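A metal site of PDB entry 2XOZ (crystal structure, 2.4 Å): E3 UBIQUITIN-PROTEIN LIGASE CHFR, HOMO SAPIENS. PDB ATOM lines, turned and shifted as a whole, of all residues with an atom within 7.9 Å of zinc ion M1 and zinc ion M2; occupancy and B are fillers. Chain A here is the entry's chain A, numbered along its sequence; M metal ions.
SG of Cys 84 is bound to zinc ion M2 (2.3 Å). SG of Cys 121 binds zinc ion M2. SG of Cys 129 binds zinc ion M2. Zinc ion M2 is bound by SG of Cys 126 (2.4 Å). Zinc ion M2 has four donor atoms within binding distance.
The nearest printed residue that does not touch zinc ion M2 is Cys 85 (4.6 Å).
SG of Cys 115 sits close to NE1 of Trp 119, 3.4 Å away. The side-chain sulfur (SG) of Cys 82 lies close to the backbone NH (N) of Cys 84. NE of Arg 123 lies within hydrogen-bond range of O of Cys 84 (3.2 Å). NE2 of Gln 87 lies within hydrogen-bond range of O of Cys 85, 3.4 Å away. The backbone NH of Cys 121 lies within hydrogen-bond range of a ring nitrogen (ND1) of His 116 (3.1 Å). N of Tyr 199 is in hydrogen-bond range of O of Cys 129 (3.2 Å). SG of Cys 126 sits close to N of Gly 128, at 3.4 Å. N of Cys 82 sits at hydrogen-bond distance from O of Gln 87 (3.0 Å).
Zinc ion M1 is bound by the side-chain sulfur of Cys 115 (2.3 Å), the side-chain sulfur of Cys 85 (2.4 Å), the side-chain sulfur of Cys 82 (2.5 Å) and the side-chain sulfur of Cys 121 (2.5 Å). Zinc ion M1 has four donor atoms within binding distance.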
ATOM      1  N   ARG A  26      19.227  31.676 -30.122  1.00  0.00           N
ATOM      2  CA  ARG A  26      18.531  32.786 -29.447  1.00  0.00           C
ATOM      3  C   ARG A  26      19.399  34.030 -29.215  1.00  0.00           C
ATOM      4  O   ARG A  26      18.884  35.148 -29.197  1.00  0.00           O
ATOM      5  CB  ARG A  26      18.001  32.320 -28.082  1.00  0.00           C
ATOM      6  CG  ARG A  26      16.755  31.459 -28.094  1.00  0.00           C
ATOM      7  CD  ARG A  26      16.178  31.344 -26.690  1.00  0.00           C
ATOM      8  NE  ARG A  26      15.824  29.959 -26.391  1.00  0.00           N
ATOM      9  CZ  ARG A  26      15.364  29.541 -25.209  1.00  0.00           C
ATOM     10  NH1 ARG A  26      15.215  30.403 -24.217  1.00  0.00           N
ATOM     11  NH2 ARG A  26      15.059  28.246 -25.027  1.00  0.00           N
ATOM     12  N   LEU A  81      24.677  21.854 -28.605  1.00  0.00           N
ATOM     13  CA  LEU A  81      23.277  21.482 -28.708  1.00  0.00           C
ATOM     14  C   LEU A  81      22.784  20.935 -27.374  1.00  0.00           C
ATOM     15  O   LEU A  81      23.357  19.980 -26.849  1.00  0.00           O
ATOM     16  CB  LEU A  81      23.092  20.439 -29.811  1.00  0.00           C
ATOM     17  CG  LEU A  81      23.473  20.900 -31.226  1.00  0.00           C
ATOM     18  CD1 LEU A  81      23.147  19.848 -32.262  1.00  0.00           C
ATOM     19  CD2 LEU A  81      22.767  22.189 -31.552  1.00  0.00           C
ATOM     20  N   CYS A  82      21.737  21.553 -26.832  1.00  0.00           N
ATOM     21  CA  CYS A  82      21.071  21.024 -25.655  1.00  0.00           C
ATOM     22  C   CYS A  82      20.669  19.585 -25.918  1.00  0.00           C
ATOM     23  O   CYS A  82      20.060  19.286 -26.937  1.00  0.00           O
ATOM     24  CB  CYS A  82      19.808  21.841 -25.308  1.00  0.00           C
ATOM     25  SG  CYS A  82      18.773  21.050 -24.050  1.00  0.00           S
ATOM     26  N   THR A  83      21.012  18.693 -24.980  1.00  0.00           N
ATOM     27  CA  THR A  83      20.750  17.266 -25.109  1.00  0.00           C
ATOM     28  C   THR A  83      19.246  16.944 -25.084  1.00  0.00           C
ATOM     29  O   THR A  83      18.800  15.894 -25.565  1.00  0.00           O
ATOM     30  CB  THR A  83      21.464  16.490 -23.975  1.00  0.00           C
ATOM     31  OG1 THR A  83      22.852  16.809 -23.989  1.00  0.00           O
ATOM     32  CG2 THR A  83      21.279  14.972 -24.106  1.00  0.00           C
ATOM     33  N   CYS A  84      18.453  17.847 -24.506  1.00  0.00           N
ATOM     34  CA  CYS A  84      17.018  17.614 -24.354  1.00  0.00           C
ATOM     35  C   CYS A  84      16.242  18.077 -25.582  1.00  0.00           C
ATOM     36  O   CYS A  84      15.521  17.290 -26.196  1.00  0.00           O
ATOM     37  CB  CYS A  84      16.485  18.309 -23.093  1.00  0.00           C
ATOM     38  SG  CYS A  84      14.684  18.386 -22.999  1.00  0.00           S
ATOM     39  N   CYS A  85      16.380  19.349 -25.932  1.00  0.00           N
ATOM     40  CA  CYS A  85      15.597  19.934 -27.013  1.00  0.00           C
ATOM     41  C   CYS A  85      16.340  20.054 -28.365  1.00  0.00           C
ATOM     42  O   CYS A  85      15.736  20.464 -29.366  1.00  0.00           O
ATOM     43  CB  CYS A  85      15.069  21.297 -26.586  1.00  0.00           C
ATOM     44  SG  CYS A  85      16.356  22.557 -26.436  1.00  0.00           S
ATOM     45  N   PHE A  86      17.618  19.705 -28.397  1.00  0.00           N
ATOM     46  CA  PHE A  86      18.437  19.800 -29.618  1.00  0.00           C
ATOM     47  C   PHE A  86      18.645  21.222 -30.189  1.00  0.00           C
ATOM     48  O   PHE A  86      19.130  21.373 -31.319  1.00  0.00           O
ATOM     49  CB  PHE A  86      17.910  18.865 -30.732  1.00  0.00           C
ATOM     50  CG  PHE A  86      17.403  17.529 -30.229  1.00  0.00           C
ATOM     51  CD1 PHE A  86      18.276  16.574 -29.713  1.00  0.00           C
ATOM     52  CD2 PHE A  86      16.045  17.237 -30.265  1.00  0.00           C
ATOM     53  CE1 PHE A  86      17.798  15.355 -29.239  1.00  0.00           C
ATOM     54  CE2 PHE A  86      15.561  16.012 -29.796  1.00  0.00           C
ATOM     55  CZ  PHE A  86      16.446  15.078 -29.282  1.00  0.00           C
ATOM     56  N   GLN A  87      18.276  22.251 -29.424  1.00  0.00           N
ATOM     57  CA  GLN A  87      18.496  23.645 -29.849  1.00  0.00           C
ATOM     58  C   GLN A  87      19.908  24.105 -29.475  1.00  0.00           C
ATOM     59  O   GLN A  87      20.405  23.765 -28.410  1.00  0.00           O
ATOM     60  CB  GLN A  87      17.458  24.596 -29.226  1.00  0.00           C
ATOM     61  CG  GLN A  87      16.004  24.284 -29.592  1.00  0.00           C
ATOM     62  CD  GLN A  87      15.814  24.181 -31.102  1.00  0.00           C
ATOM     63  OE1 GLN A  87      15.895  25.188 -31.816  1.00  0.00           O
ATOM     64  NE2 GLN A  87      15.562  22.965 -31.592  1.00  0.00           N
ATOM     65  N   PRO A  88      20.559  24.890 -30.358  1.00  0.00           N
ATOM     66  CA  PRO A  88      21.910  25.377 -30.053  1.00  0.00           C
ATOM     67  C   PRO A  88      21.905  26.478 -29.001  1.00  0.00           C
ATOM     68  O   PRO A  88      21.000  27.300 -28.935  1.00  0.00           O
ATOM     69  CB  PRO A  88      22.373  25.944 -31.382  1.00  0.00           C
ATOM     70  CG  PRO A  88      21.091  26.401 -32.037  1.00  0.00           C
ATOM     71  CD  PRO A  88      20.113  25.307 -31.705  1.00  0.00           C
ATOM     72  N   MET A  89      22.931  26.460 -28.153  1.00  0.00           N
ATOM     73  CA  MET A  89      23.167  27.517 -27.186  1.00  0.00           C
ATOM     74  C   MET A  89      24.638  27.829 -27.263  1.00  0.00           C
ATOM     75  O   MET A  89      25.426  27.023 -27.746  1.00  0.00           O
ATOM     76  CB  MET A  89      22.774  27.071 -25.777  1.00  0.00           C
ATOM     77  CG  MET A  89      23.548  25.860 -25.290  1.00  0.00           C
ATOM     78  SD  MET A  89      22.977  25.272 -23.692  1.00  0.00           S
ATOM     79  CE  MET A  89      23.862  23.736 -23.572  1.00  0.00           C
ATOM     80  N   PRO A 113      25.357  18.421 -22.271  1.00  0.00           N
ATOM     81  CA  PRO A 113      24.855  19.793 -22.089  1.00  0.00           C
ATOM     82  C   PRO A 113      23.330  19.911 -22.134  1.00  0.00           C
ATOM     83  O   PRO A 113      22.665  19.234 -22.920  1.00  0.00           O
ATOM     84  CB  PRO A 113      25.488  20.562 -23.253  1.00  0.00           C
ATOM     85  CG  PRO A 113      25.707  19.523 -24.325  1.00  0.00           C
ATOM     86  CD  PRO A 113      25.772  18.169 -23.663  1.00  0.00           C
ATOM     87  N   PHE A 114      22.799  20.786 -21.282  1.00  0.00           N
ATOM     88  CA  PHE A 114      21.372  21.106 -21.266  1.00  0.00           C
ATOM     89  C   PHE A 114      21.159  22.604 -21.152  1.00  0.00           C
ATOM     90  O   PHE A 114      21.903  23.307 -20.467  1.00  0.00           O
ATOM     91  CB  PHE A 114      20.687  20.367 -20.126  1.00  0.00           C
ATOM     92  CG  PHE A 114      20.772  18.866 -20.237  1.00  0.00           C
ATOM     93  CD1 PHE A 114      19.716  18.149 -20.758  1.00  0.00           C
ATOM     94  CD2 PHE A 114      21.923  18.204 -19.844  1.00  0.00           C
ATOM     95  CE1 PHE A 114      19.800  16.769 -20.870  1.00  0.00           C
ATOM     96  CE2 PHE A 114      22.006  16.824 -19.956  1.00  0.00           C
ATOM     97  CZ  PHE A 114      20.944  16.107 -20.469  1.00  0.00           C
ATOM     98  N   CYS A 115      20.137  23.118 -21.830  1.00  0.00           N
ATOM     99  CA  CYS A 115      19.960  24.567 -21.871  1.00  0.00           C
ATOM    100  C   CYS A 115      19.076  25.140 -20.740  1.00  0.00           C
ATOM    101  O   CYS A 115      18.971  26.360 -20.587  1.00  0.00           O
ATOM    102  CB  CYS A 115      19.398  24.997 -23.229  1.00  0.00           C
ATOM    103  SG  CYS A 115      17.599  24.773 -23.394  1.00  0.00           S
ATOM    104  N   HIS A 116      18.447  24.286 -19.950  1.00  0.00           N
ATOM    105  CA  HIS A 116      17.373  24.767 -19.090  1.00  0.00           C
ATOM    106  C   HIS A 116      17.722  25.849 -18.059  1.00  0.00           C
ATOM    107  O   HIS A 116      16.972  26.805 -17.884  1.00  0.00           O
ATOM    108  CB  HIS A 116      16.647  23.627 -18.367  1.00  0.00           C
ATOM    109  CG  HIS A 116      15.434  24.090 -17.653  1.00  0.00           C
ATOM    110  ND1 HIS A 116      14.302  24.529 -18.309  1.00  0.00           N
ATOM    111  CD2 HIS A 116      15.173  24.252 -16.330  1.00  0.00           C
ATOM    112  CE1 HIS A 116      13.396  24.905 -17.432  1.00  0.00           C
ATOM    113  NE2 HIS A 116      13.902  24.742 -16.214  1.00  0.00           N
ATOM    114  N   LEU A 117      18.824  25.680 -17.333  1.00  0.00           N
ATOM    115  CA  LEU A 117      19.222  26.673 -16.338  1.00  0.00           C
ATOM    116  C   LEU A 117      19.783  27.899 -17.013  1.00  0.00           C
ATOM    117  O   LEU A 117      19.734  29.004 -16.463  1.00  0.00           O
ATOM    118  CB  LEU A 117      20.275  26.105 -15.377  1.00  0.00           C
ATOM    119  CG  LEU A 117      19.704  25.078 -14.396  1.00  0.00           C
ATOM    120  CD1 LEU A 117      20.781  24.564 -13.474  1.00  0.00           C
ATOM    121  CD2 LEU A 117      18.572  25.728 -13.599  1.00  0.00           C
ATOM    122  N   TRP A 119      18.834  29.371 -20.010  1.00  0.00           N
ATOM    123  CA  TRP A 119      17.817  30.270 -20.553  1.00  0.00           C
ATOM    124  C   TRP A 119      16.410  29.687 -20.684  1.00  0.00           C
ATOM    125  O   TRP A 119      15.565  30.267 -21.345  1.00  0.00           O
ATOM    126  CB  TRP A 119      18.270  30.860 -21.900  1.00  0.00           C
ATOM    127  CG  TRP A 119      18.449  29.862 -23.022  1.00  0.00           C
ATOM    128  CD1 TRP A 119      17.933  28.608 -23.087  1.00  0.00           C
ATOM    129  CD2 TRP A 119      19.168  30.077 -24.256  1.00  0.00           C
ATOM    130  NE1 TRP A 119      18.299  28.009 -24.275  1.00  0.00           N
ATOM    131  CE2 TRP A 119      19.053  28.895 -25.005  1.00  0.00           C
ATOM    132  CE3 TRP A 119      19.888  31.143 -24.789  1.00  0.00           C
ATOM    133  CZ2 TRP A 119      19.640  28.748 -26.265  1.00  0.00           C
ATOM    134  CZ3 TRP A 119      20.475  31.002 -26.037  1.00  0.00           C
ATOM    135  CH2 TRP A 119      20.359  29.818 -26.761  1.00  0.00           C
ATOM    136  N   GLY A 120      16.160  28.556 -20.037  1.00  0.00           N
ATOM    137  CA  GLY A 120      14.828  27.976 -20.034  1.00  0.00           C
ATOM    138  C   GLY A 120      14.600  27.153 -21.286  1.00  0.00           C
ATOM    139  O   GLY A 120      14.639  27.671 -22.401  1.00  0.00           O
ATOM    140  N   CYS A 121      14.410  25.859 -21.092  1.00  0.00           N
ATOM    141  CA  CYS A 121      14.246  24.938 -22.203  1.00  0.00           C
ATOM    142  C   CYS A 121      12.756  24.680 -22.401  1.00  0.00           C
ATOM    143  O   CYS A 121      11.973  24.753 -21.450  1.00  0.00           O
ATOM    144  CB  CYS A 121      14.989  23.630 -21.890  1.00  0.00           C
ATOM    145  SG  CYS A 121      14.759  22.295 -23.072  1.00  0.00           S
ATOM    146  N   THR A 122      12.350  24.383 -23.630  1.00  0.00           N
ATOM    147  CA  THR A 122      10.949  24.069 -23.891  1.00  0.00           C
ATOM    148  C   THR A 122      10.802  22.931 -24.887  1.00  0.00           C
ATOM    149  O   THR A 122      11.334  22.973 -25.980  1.00  0.00           O
ATOM    150  CB  THR A 122      10.182  25.299 -24.434  1.00  0.00           C
ATOM    151  OG1 THR A 122      10.245  26.345 -23.462  1.00  0.00           O
ATOM    152  CG2 THR A 122       8.725  24.943 -24.718  1.00  0.00           C
ATOM    153  N   ARG A 123      10.051  21.927 -24.485  1.00  0.00           N
ATOM    154  CA  ARG A 123       9.748  20.802 -25.345  1.00  0.00           C
ATOM    155  C   ARG A 123       8.671  20.018 -24.638  1.00  0.00           C
ATOM    156  O   ARG A 123       8.689  19.903 -23.409  1.00  0.00           O
ATOM    157  CB  ARG A 123      10.983  19.899 -25.546  1.00  0.00           C
ATOM    158  CG  ARG A 123      10.688  18.683 -26.411  1.00  0.00           C
ATOM    159  CD  ARG A 123      11.898  17.818 -26.716  1.00  0.00           C
ATOM    160  NE  ARG A 123      12.434  17.182 -25.514  1.00  0.00           N
ATOM    161  CZ  ARG A 123      11.921  16.089 -24.951  1.00  0.00           C
ATOM    162  NH1 ARG A 123      10.840  15.506 -25.465  1.00  0.00           N
ATOM    163  NH2 ARG A 123      12.482  15.584 -23.855  1.00  0.00           N
ATOM    164  N   GLY A 125       7.431  17.083 -23.063  1.00  0.00           N
ATOM    165  CA  GLY A 125       8.142  15.960 -22.462  1.00  0.00           C
ATOM    166  C   GLY A 125       9.214  16.407 -21.490  1.00  0.00           C
ATOM    167  O   GLY A 125       9.680  15.613 -20.663  1.00  0.00           O
ATOM    168  N   CYS A 126       9.602  17.674 -21.586  1.00  0.00           N
ATOM    169  CA  CYS A 126      10.618  18.257 -20.718  1.00  0.00           C
ATOM    170  C   CYS A 126       9.922  18.988 -19.565  1.00  0.00           C
ATOM    171  O   CYS A 126       9.091  19.860 -19.792  1.00  0.00           O
ATOM    172  CB  CYS A 126      11.541  19.202 -21.513  1.00  0.00           C
ATOM    173  SG  CYS A 126      12.567  20.360 -20.549  1.00  0.00           S
ATOM    174  N   TYR A 127      10.263  18.616 -18.345  1.00  0.00           N
ATOM    175  CA  TYR A 127       9.654  19.188 -17.155  1.00  0.00           C
ATOM    176  C   TYR A 127      10.524  20.312 -16.619  1.00  0.00           C
ATOM    177  O   TYR A 127      10.153  20.988 -15.653  1.00  0.00           O
ATOM    178  CB  TYR A 127       9.526  18.118 -16.080  1.00  0.00           C
ATOM    179  CG  TYR A 127       8.888  16.837 -16.558  1.00  0.00           C
ATOM    180  CD1 TYR A 127       7.646  16.851 -17.180  1.00  0.00           C
ATOM    181  CD2 TYR A 127       9.530  15.617 -16.375  1.00  0.00           C
ATOM    182  CE1 TYR A 127       7.050  15.680 -17.613  1.00  0.00           C
ATOM    183  CE2 TYR A 127       8.946  14.434 -16.825  1.00  0.00           C
ATOM    184  CZ  TYR A 127       7.692  14.469 -17.442  1.00  0.00           C
ATOM    185  OH  TYR A 127       7.091  13.305 -17.878  1.00  0.00           O
ATOM    186  N   GLY A 128      11.678  20.494 -17.257  1.00  0.00           N
ATOM    187  CA  GLY A 128      12.783  21.279 -16.703  1.00  0.00           C
ATOM    188  C   GLY A 128      13.980  20.359 -16.493  1.00  0.00           C
ATOM    189  O   GLY A 128      14.156  19.771 -15.422  1.00  0.00           O
ATOM    190  N   CYS A 129      14.829  20.273 -17.521  1.00  0.00           N
ATOM    191  CA  CYS A 129      15.732  19.159 -17.733  1.00  0.00           C
ATOM    192  C   CYS A 129      17.086  19.254 -17.039  1.00  0.00           C
ATOM    193  O   CYS A 129      17.914  18.374 -17.183  1.00  0.00           O
ATOM    194  CB  CYS A 129      15.960  18.973 -19.249  1.00  0.00           C
ATOM    195  SG  CYS A 129      16.514  20.467 -20.141  1.00  0.00           S
ATOM    196  N   LEU A 130      17.307  20.347 -16.307  1.00  0.00           N
ATOM    197  CA  LEU A 130      18.516  20.530 -15.512  1.00  0.00           C
ATOM    198  C   LEU A 130      18.151  21.285 -14.255  1.00  0.00           C
ATOM    199  O   LEU A 130      17.541  22.337 -14.304  1.00  0.00           O
ATOM    200  CB  LEU A 130      19.592  21.299 -16.298  1.00  0.00           C
ATOM    201  CG  LEU A 130      21.028  21.253 -15.746  1.00  0.00           C
ATOM    202  CD1 LEU A 130      21.633  19.851 -15.902  1.00  0.00           C
ATOM    203  CD2 LEU A 130      21.926  22.327 -16.407  1.00  0.00           C
ATOM    204  N   TYR A 199      17.313  15.490 -16.022  1.00  0.00           N
ATOM    205  CA  TYR A 199      16.145  14.646 -15.821  1.00  0.00           C
ATOM    206  C   TYR A 199      16.506  13.160 -15.732  1.00  0.00           C
ATOM    207  O   TYR A 199      16.089  12.454 -14.813  1.00  0.00           O
ATOM    208  CB  TYR A 199      15.151  14.856 -16.966  1.00  0.00           C
ATOM    209  CG  TYR A 199      14.105  13.772 -16.975  1.00  0.00           C
ATOM    210  CD1 TYR A 199      13.093  13.770 -16.032  1.00  0.00           C
ATOM    211  CD2 TYR A 199      14.150  12.738 -17.901  1.00  0.00           C
ATOM    212  CE1 TYR A 199      12.137  12.770 -16.014  1.00  0.00           C
ATOM    213  CE2 TYR A 199      13.183  11.738 -17.892  1.00  0.00           C
ATOM    214  CZ  TYR A 199      12.181  11.764 -16.937  1.00  0.00           C
ATOM    215  OH  TYR A 199      11.219  10.777 -16.910  1.00  0.00           O
HETATM  216 ZN    ZN M   1      16.954  22.700 -24.140  1.00  0.00          ZN
HETATM  217 ZN    ZN M   2      14.698  20.306 -21.729  1.00  0.00          ZN
